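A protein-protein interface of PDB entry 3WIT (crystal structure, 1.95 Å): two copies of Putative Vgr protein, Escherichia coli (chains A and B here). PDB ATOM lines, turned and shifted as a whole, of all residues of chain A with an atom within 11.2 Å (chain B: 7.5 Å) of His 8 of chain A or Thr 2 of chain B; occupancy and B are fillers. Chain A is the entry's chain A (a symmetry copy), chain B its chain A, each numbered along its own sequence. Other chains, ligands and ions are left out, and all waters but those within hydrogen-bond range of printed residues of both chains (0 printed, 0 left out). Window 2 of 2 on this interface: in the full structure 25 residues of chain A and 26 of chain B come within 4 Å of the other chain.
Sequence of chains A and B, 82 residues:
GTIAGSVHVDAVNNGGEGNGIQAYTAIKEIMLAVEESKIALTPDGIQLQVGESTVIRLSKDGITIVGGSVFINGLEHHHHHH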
ATOM      1  N   GLY A   5     -28.605  38.385  28.380  1.00  0.00           N
ATOM      2  CA  GLY A   5     -29.961  37.877  28.189  1.00  0.00           C
ATOM      3  C   GLY A   5     -30.050  36.392  28.453  1.00  0.00           C
ATOM      4  O   GLY A   5     -29.083  35.663  28.229  1.00  0.00           O
ATOM      5  N   SER A   6     -31.187  35.956  28.974  1.00  0.00           N
ATOM      6  CA  SER A   6     -31.439  34.544  29.202  1.00  0.00           C
ATOM      7  C   SER A   6     -32.818  34.333  28.618  1.00  0.00           C
ATOM      8  O   SER A   6     -33.750  35.066  28.965  1.00  0.00           O
ATOM      9  CB  SER A   6     -31.435  34.260  30.704  1.00  0.00           C
ATOM     10  OG  SER A   6     -31.908  32.952  30.968  1.00  0.00           O
ATOM     11  N   VAL A   7     -32.946  33.388  27.679  1.00  0.00           N
ATOM     12  CA  VAL A   7     -34.235  33.097  27.043  1.00  0.00           C
ATOM     13  C   VAL A   7     -34.557  31.588  27.035  1.00  0.00           C
ATOM     14  O   VAL A   7     -33.677  30.775  26.800  1.00  0.00           O
ATOM     15  CB  VAL A   7     -34.308  33.632  25.587  1.00  0.00           C
ATOM     16  CG1 VAL A   7     -35.653  33.320  24.995  1.00  0.00           C
ATOM     17  CG2 VAL A   7     -34.137  35.135  25.550  1.00  0.00           C
ATOM     18  N   HIS A   8     -35.810  31.232  27.316  1.00  0.00           N
ATOM     19  CA  HIS A   8     -36.288  29.858  27.188  1.00  0.00           C
ATOM     20  C   HIS A   8     -37.652  29.930  26.508  1.00  0.00           C
ATOM     21  O   HIS A   8     -38.673  30.155  27.163  1.00  0.00           O
ATOM     22  CB  HIS A   8     -36.372  29.165  28.550  1.00  0.00           C
ATOM     23  CG  HIS A   8     -36.655  27.692  28.481  1.00  0.00           C
ATOM     24  ND1 HIS A   8     -37.596  27.146  27.635  1.00  0.00           N
ATOM     25  CD2 HIS A   8     -36.128  26.653  29.176  1.00  0.00           C
ATOM     26  CE1 HIS A   8     -37.636  25.837  27.809  1.00  0.00           C
ATOM     27  NE2 HIS A   8     -36.755  25.512  28.739  1.00  0.00           N
ATOM     28  N   VAL A   9     -37.629  29.733  25.188  1.00  0.00           N
ATOM     29  CA  VAL A   9     -38.719  30.047  24.242  1.00  0.00           C
ATOM     30  C   VAL A   9     -39.334  31.436  24.419  1.00  0.00           C
ATOM     31  O   VAL A   9     -38.911  32.394  23.766  1.00  0.00           O
ATOM     32  CB  VAL A   9     -39.814  28.960  24.184  1.00  0.00           C
ATOM     33  CG1 VAL A   9     -40.890  29.345  23.175  1.00  0.00           C
ATOM     34  CG2 VAL A   9     -39.187  27.628  23.815  1.00  0.00           C
ATOM     35  N   ILE A  27     -34.234  29.459  21.107  1.00  0.00           N
ATOM     36  CA  ILE A  27     -35.298  29.211  22.069  1.00  0.00           C
ATOM     37  C   ILE A  27     -34.820  28.817  23.488  1.00  0.00           C
ATOM     38  O   ILE A  27     -35.582  28.942  24.428  1.00  0.00           O
ATOM     39  CB  ILE A  27     -36.307  28.173  21.542  1.00  0.00           C
ATOM     40  CG1 ILE A  27     -35.728  26.754  21.633  1.00  0.00           C
ATOM     41  CG2 ILE A  27     -36.723  28.534  20.117  1.00  0.00           C
ATOM     42  CD1 ILE A  27     -36.778  25.657  21.709  1.00  0.00           C
ATOM     43  N   LYS A  28     -33.593  28.315  23.642  1.00  0.00           N
ATOM     44  CA  LYS A  28     -32.975  28.193  24.972  1.00  0.00           C
ATOM     45  C   LYS A  28     -31.561  28.707  24.832  1.00  0.00           C
ATOM     46  O   LYS A  28     -30.705  28.058  24.224  1.00  0.00           O
ATOM     47  CB  LYS A  28     -32.863  26.741  25.425  1.00  0.00           C
ATOM     48  CG  LYS A  28     -34.157  25.959  25.534  1.00  0.00           C
ATOM     49  CD  LYS A  28     -33.834  24.579  26.127  1.00  0.00           C
ATOM     50  CE  LYS A  28     -35.069  23.797  26.522  1.00  0.00           C
ATOM     51  NZ  LYS A  28     -34.701  22.729  27.493  1.00  0.00           N
ATOM     52  N   GLU A  29     -31.273  29.868  25.398  1.00  0.00           N
ATOM     53  CA  GLU A  29     -29.963  30.442  25.159  1.00  0.00           C
ATOM     54  C   GLU A  29     -29.671  31.421  26.266  1.00  0.00           C
ATOM     55  O   GLU A  29     -30.607  32.053  26.761  1.00  0.00           O
ATOM     56  CB  GLU A  29     -30.011  31.175  23.828  1.00  0.00           C
ATOM     57  CG  GLU A  29     -28.728  31.852  23.441  1.00  0.00           C
ATOM     58  CD  GLU A  29     -28.757  32.309  21.983  1.00  0.00           C
ATOM     59  OE1 GLU A  29     -27.721  32.833  21.491  1.00  0.00           O
ATOM     60  OE2 GLU A  29     -29.824  32.135  21.341  1.00  0.00           O
ATOM     61  N   ILE A  30     -28.405  31.525  26.659  1.00  0.00           N
ATOM     62  CA  ILE A  30     -27.956  32.636  27.512  1.00  0.00           C
ATOM     63  C   ILE A  30     -26.868  33.324  26.700  1.00  0.00           C
ATOM     64  O   ILE A  30     -26.006  32.641  26.121  1.00  0.00           O
ATOM     65  CB  ILE A  30     -27.340  32.116  28.809  1.00  0.00           C
ATOM     66  CG1 ILE A  30     -28.422  31.575  29.717  1.00  0.00           C
ATOM     67  CG2 ILE A  30     -26.546  33.249  29.533  1.00  0.00           C
ATOM     68  CD1 ILE A  30     -27.892  30.707  30.859  1.00  0.00           C
ATOM     69  N   MET A  31     -26.916  34.651  26.602  1.00  0.00           N
ATOM     70  CA  MET A  31     -25.889  35.388  25.858  1.00  0.00           C
ATOM     71  C   MET A  31     -25.351  36.563  26.677  1.00  0.00           C
ATOM     72  O   MET A  31     -26.128  37.333  27.244  1.00  0.00           O
ATOM     73  CB  MET A  31     -26.485  35.910  24.542  1.00  0.00           C
ATOM     74  CG  MET A  31     -25.674  36.993  23.869  1.00  0.00           C
ATOM     75  SD  MET A  31     -24.183  36.187  22.947  1.00  0.00           S
ATOM     76  CE  MET A  31     -25.145  35.637  21.353  1.00  0.00           C
ATOM     77  N   ALA A  40     -21.735  32.620  24.858  1.00  0.00           N
ATOM     78  CA  ALA A  40     -23.085  32.094  24.599  1.00  0.00           C
ATOM     79  C   ALA A  40     -23.203  30.670  25.102  1.00  0.00           C
ATOM     80  O   ALA A  40     -22.279  29.867  24.933  1.00  0.00           O
ATOM     81  CB  ALA A  40     -23.402  32.129  23.109  1.00  0.00           C
ATOM     82  N   LEU A  41     -24.334  30.357  25.726  1.00  0.00           N
ATOM     83  CA  LEU A  41     -24.616  28.989  26.137  1.00  0.00           C
ATOM     84  C   LEU A  41     -25.886  28.538  25.449  1.00  0.00           C
ATOM     85  O   LEU A  41     -26.898  29.267  25.439  1.00  0.00           O
ATOM     86  CB  LEU A  41     -24.794  28.902  27.662  1.00  0.00           C
ATOM     87  CG  LEU A  41     -23.659  29.330  28.595  1.00  0.00           C
ATOM     88  CD1 LEU A  41     -23.715  30.808  28.916  1.00  0.00           C
ATOM     89  CD2 LEU A  41     -23.778  28.507  29.889  1.00  0.00           C
ATOM     90  N   THR A  42     -25.852  27.334  24.870  1.00  0.00           N
ATOM     91  CA  THR A  42     -27.023  26.771  24.219  1.00  0.00           C
ATOM     92  C   THR A  42     -27.071  25.272  24.572  1.00  0.00           C
ATOM     93  O   THR A  42     -26.162  24.761  25.214  1.00  0.00           O
ATOM     94  CB  THR A  42     -26.911  26.919  22.690  1.00  0.00           C
ATOM     95  OG1 THR A  42     -25.685  26.313  22.237  1.00  0.00           O
ATOM     96  CG2 THR A  42     -26.952  28.394  22.277  1.00  0.00           C
ATOM     97  N   PRO A  43     -28.099  24.560  24.124  1.00  0.00           N
ATOM     98  CA  PRO A  43     -28.045  23.132  24.428  1.00  0.00           C
ATOM     99  C   PRO A  43     -26.854  22.430  23.740  1.00  0.00           C
ATOM    100  O   PRO A  43     -26.496  21.336  24.146  1.00  0.00           O
ATOM    101  CB  PRO A  43     -29.363  22.640  23.883  1.00  0.00           C
ATOM    102  CG  PRO A  43     -30.255  23.808  23.985  1.00  0.00           C
ATOM    103  CD  PRO A  43     -29.394  24.921  23.529  1.00  0.00           C
ATOM    104  N   ASP A  44     -26.265  23.055  22.717  1.00  0.00           N
ATOM    105  CA  ASP A  44     -25.150  22.453  21.984  1.00  0.00           C
ATOM    106  C   ASP A  44     -23.815  22.682  22.647  1.00  0.00           C
ATOM    107  O   ASP A  44     -22.838  21.976  22.348  1.00  0.00           O
ATOM    108  CB  ASP A  44     -25.059  23.040  20.597  1.00  0.00           C
ATOM    109  CG  ASP A  44     -26.016  22.394  19.635  1.00  0.00           C
ATOM    110  OD1 ASP A  44     -26.662  21.373  19.990  1.00  0.00           O
ATOM    111  OD2 ASP A  44     -26.100  22.904  18.502  1.00  0.00           O
ATOM    112  N   GLY A  45     -23.743  23.687  23.514  1.00  0.00           N
ATOM    113  CA  GLY A  45     -22.509  23.911  24.261  1.00  0.00           C
ATOM    114  C   GLY A  45     -22.260  25.362  24.619  1.00  0.00           C
ATOM    115  O   GLY A  45     -23.197  26.159  24.783  1.00  0.00           O
ATOM    116  N   GLY B   1     -33.768  22.404  30.862  1.00  0.00           N
ATOM    117  CA  GLY B   1     -34.227  23.693  31.342  1.00  0.00           C
ATOM    118  C   GLY B   1     -33.122  24.725  31.248  1.00  0.00           C
ATOM    119  O   GLY B   1     -32.040  24.448  30.726  1.00  0.00           O
ATOM    120  N   THR B   2     -33.400  25.934  31.737  1.00  0.00           N
ATOM    121  CA  THR B   2     -32.424  27.028  31.748  1.00  0.00           C
ATOM    122  C   THR B   2     -32.483  27.817  33.061  1.00  0.00           C
ATOM    123  O   THR B   2     -33.559  28.049  33.603  1.00  0.00           O
ATOM    124  CB  THR B   2     -32.591  28.006  30.570  1.00  0.00           C
ATOM    125  OG1 THR B   2     -33.906  28.567  30.596  1.00  0.00           O
ATOM    126  CG2 THR B   2     -32.404  27.297  29.255  1.00  0.00           C
ATOM    127  N   ILE B   3     -31.317  28.205  33.565  1.00  0.00           N
ATOM    128  CA  ILE B   3     -31.194  28.896  34.856  1.00  0.00           C
ATOM    129  C   ILE B   3     -30.138  29.974  34.726  1.00  0.00           C
ATOM    130  O   ILE B   3     -29.052  29.685  34.270  1.00  0.00           O
ATOM    131  CB  ILE B   3     -30.664  27.927  35.942  1.00  0.00           C
ATOM    132  CG1 ILE B   3     -31.725  26.923  36.363  1.00  0.00           C
ATOM    133  CG2 ILE B   3     -30.172  28.688  37.156  1.00  0.00           C
ATOM    134  CD1 ILE B   3     -31.238  25.962  37.420  1.00  0.00           C
ATOM    135  N   ALA B   4     -30.419  31.214  35.131  1.00  0.00           N
ATOM    136  CA  ALA B   4     -29.337  32.184  35.261  1.00  0.00           C
ATOM    137  C   ALA B   4     -29.582  32.847  36.603  1.00  0.00           C
ATOM    138  O   ALA B   4     -30.672  33.387  36.817  1.00  0.00           O
ATOM    139  CB  ALA B   4     -29.399  33.204  34.158  1.00  0.00           C
ATOM    140  N   LEU B  32     -24.928  29.922  35.325  1.00  0.00           N
ATOM    141  CA  LEU B  32     -25.589  30.106  34.033  1.00  0.00           C
ATOM    142  C   LEU B  32     -25.710  28.707  33.448  1.00  0.00           C
ATOM    143  O   LEU B  32     -24.708  28.034  33.261  1.00  0.00           O
ATOM    144  CB  LEU B  32     -24.721  30.926  33.103  1.00  0.00           C
ATOM    145  CG  LEU B  32     -24.325  32.315  33.588  1.00  0.00           C
ATOM    146  CD1 LEU B  32     -23.398  32.990  32.572  1.00  0.00           C
ATOM    147  CD2 LEU B  32     -25.607  33.080  33.760  1.00  0.00           C
ATOM    148  N   ALA B  33     -26.918  28.267  33.152  1.00  0.00           N
ATOM    149  CA  ALA B  33     -27.116  26.921  32.645  1.00  0.00           C
ATOM    150  C   ALA B  33     -28.184  26.868  31.541  1.00  0.00           C
ATOM    151  O   ALA B  33     -29.264  27.462  31.657  1.00  0.00           O
ATOM    152  CB  ALA B  33     -27.489  25.994  33.798  1.00  0.00           C
ATOM    153  N   VAL B  34     -27.866  26.156  30.465  1.00  0.00           N
ATOM    154  CA  VAL B  34     -28.837  25.820  29.460  1.00  0.00           C
ATOM    155  C   VAL B  34     -28.678  24.304  29.252  1.00  0.00           C
ATOM    156  O   VAL B  34     -27.609  23.849  28.834  1.00  0.00           O
ATOM    157  CB  VAL B  34     -28.536  26.588  28.138  1.00  0.00           C
ATOM    158  CG1 VAL B  34     -29.495  26.154  27.074  1.00  0.00           C
ATOM    159  CG2 VAL B  34     -28.653  28.115  28.348  1.00  0.00           C
ATOM    160  N   GLU B  35     -29.696  23.527  29.586  1.00  0.00           N
ATOM    161  CA  GLU B  35     -29.574  22.050  29.642  1.00  0.00           C
ATOM    162  C   GLU B  35     -28.254  21.619  30.275  1.00  0.00           C
ATOM    163  O   GLU B  35     -27.978  21.956  31.426  1.00  0.00           O
ATOM    164  CB  GLU B  35     -29.656  21.429  28.256  1.00  0.00           C
ATOM    165  CG  GLU B  35     -30.533  22.188  27.323  1.00  0.00           C
ATOM    166  CD  GLU B  35     -31.842  21.521  27.124  1.00  0.00           C
ATOM    167  OE1 GLU B  35     -32.706  21.663  28.018  1.00  0.00           O
ATOM    168  OE2 GLU B  35     -32.006  20.850  26.082  1.00  0.00           O
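OE2 of Glu 35 of chain B lies within salt-bridge range of NZ of Lys 28 of chain A (3.6 Å).
The backbone NH (N) of Leu 41 of chain A is in hydrogen-bond range of the backbone carbonyl oxygen (O) of Ile 30 of chain A, at 2.9 Å. O of Ile 3 of chain B lies within hydrogen-bond range of N of Ala 33 of chain B (2.8 Å). The backbone carbonyl oxygen (O) of Gly 1 of chain B is in hydrogen-bond range of the backbone NH (N) of Glu 35 of chain B (2.8 Å). The side-chain hydroxyl (OG1) of Thr 42 of chain A lies close to the backbone NH (N) of Asp 44 of chain A, 3.3 Å away.
Among the printed residues, pairs that only touch across the chains: His 8 of chain A with Thr 2 of chain B, Lys 28 of chain A with Gly 1 of chain B, Lys 28 of chain A with Thr 2 of chain B, Lys 28 of chain A with Val 34 of chain B, Ile 30 of chain A with Ile 3 of chain B, Ile 30 of chain A with Leu 32 of chain B, Ile 30 of chain A with Ala 33 of chain B, Ile 30 of chain A with Val 34 of chain B, Leu 41 of chain A with Leu 32 of chain B, Leu 41 of chain A with Val 34 of chain B, Thr 42 of chain A with Val 34 of chain B, Pro 43 of chain A with Val 34 of chain B and Pro 43 of chain A with Glu 35 of chain B.
His 8 of chain A touches just one residue of chain B: Thr 2. Printed residues of chain B within 4 Å of Lys 28 of chain A: Gly 1, Thr 2, Val 34 and Glu 35. Of the printed residues of chain B, Ile 30 of chain A touches Ile 3, Leu 32, Ala 33 and Val 34. Printed residues of chain B within 4 Å of Leu 41 of chain A: Leu 32 (3.5 Å) and Val 34 (3.6 Å). Of the printed residues of chain B, Thr 42 of chain A touches Val 34. Printed residues of chain B within 4 Å of Pro 43 of chain A: Val 34 (3.6 Å) and Glu 35 (3.7 Å). Printed residues of chain A within 4 Å of Gly 1 of chain B: Lys 28 (3.5 Å). Of chain A, only His 8 and Lys 28 come within 4 Å of Thr 2 of chain B. Ile 3 of chain B touches just one residue of chain A: Ile 30. No residue of chain A comes within 4 Å of Ala 4 of chain B. Of chain A, only Ile 30 (3.5 Å) comes within 4 Å of Ala 33 of chain B. Of chain A, only Lys 28 (3.6 Å), Ile 30 (3.7 Å), Leu 41 (3.6 Å), Thr 42 (3.6 Å) and Pro 43 (3.6 Å) come within 4 Å of Val 34 of chain B. The nearest residue of chain B that does not touch His 8 of chain A is Gly 1 of chain B (4.1 Å).
Hydrophobic or aromatic side chains of chain B that line the printed part of chain A: Leu 32 and Val 34. Hydrophobic or aromatic side chains of chain A that line the printed part of chain B: His 8, Ile 30, Leu 41 and Pro 43. Along chain A the printed residues that touch a printed residue of chain B span positions 8 to 43. Among the printed residues, 14 pairs touch across the chains. Among the printed residues, Asp or Glu carboxylates within 4 Å of a Lys or Arg side-chain nitrogen of the other chain: Lys 28 of chain A with Glu 35 of chain B.
No position is printed for both chains.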
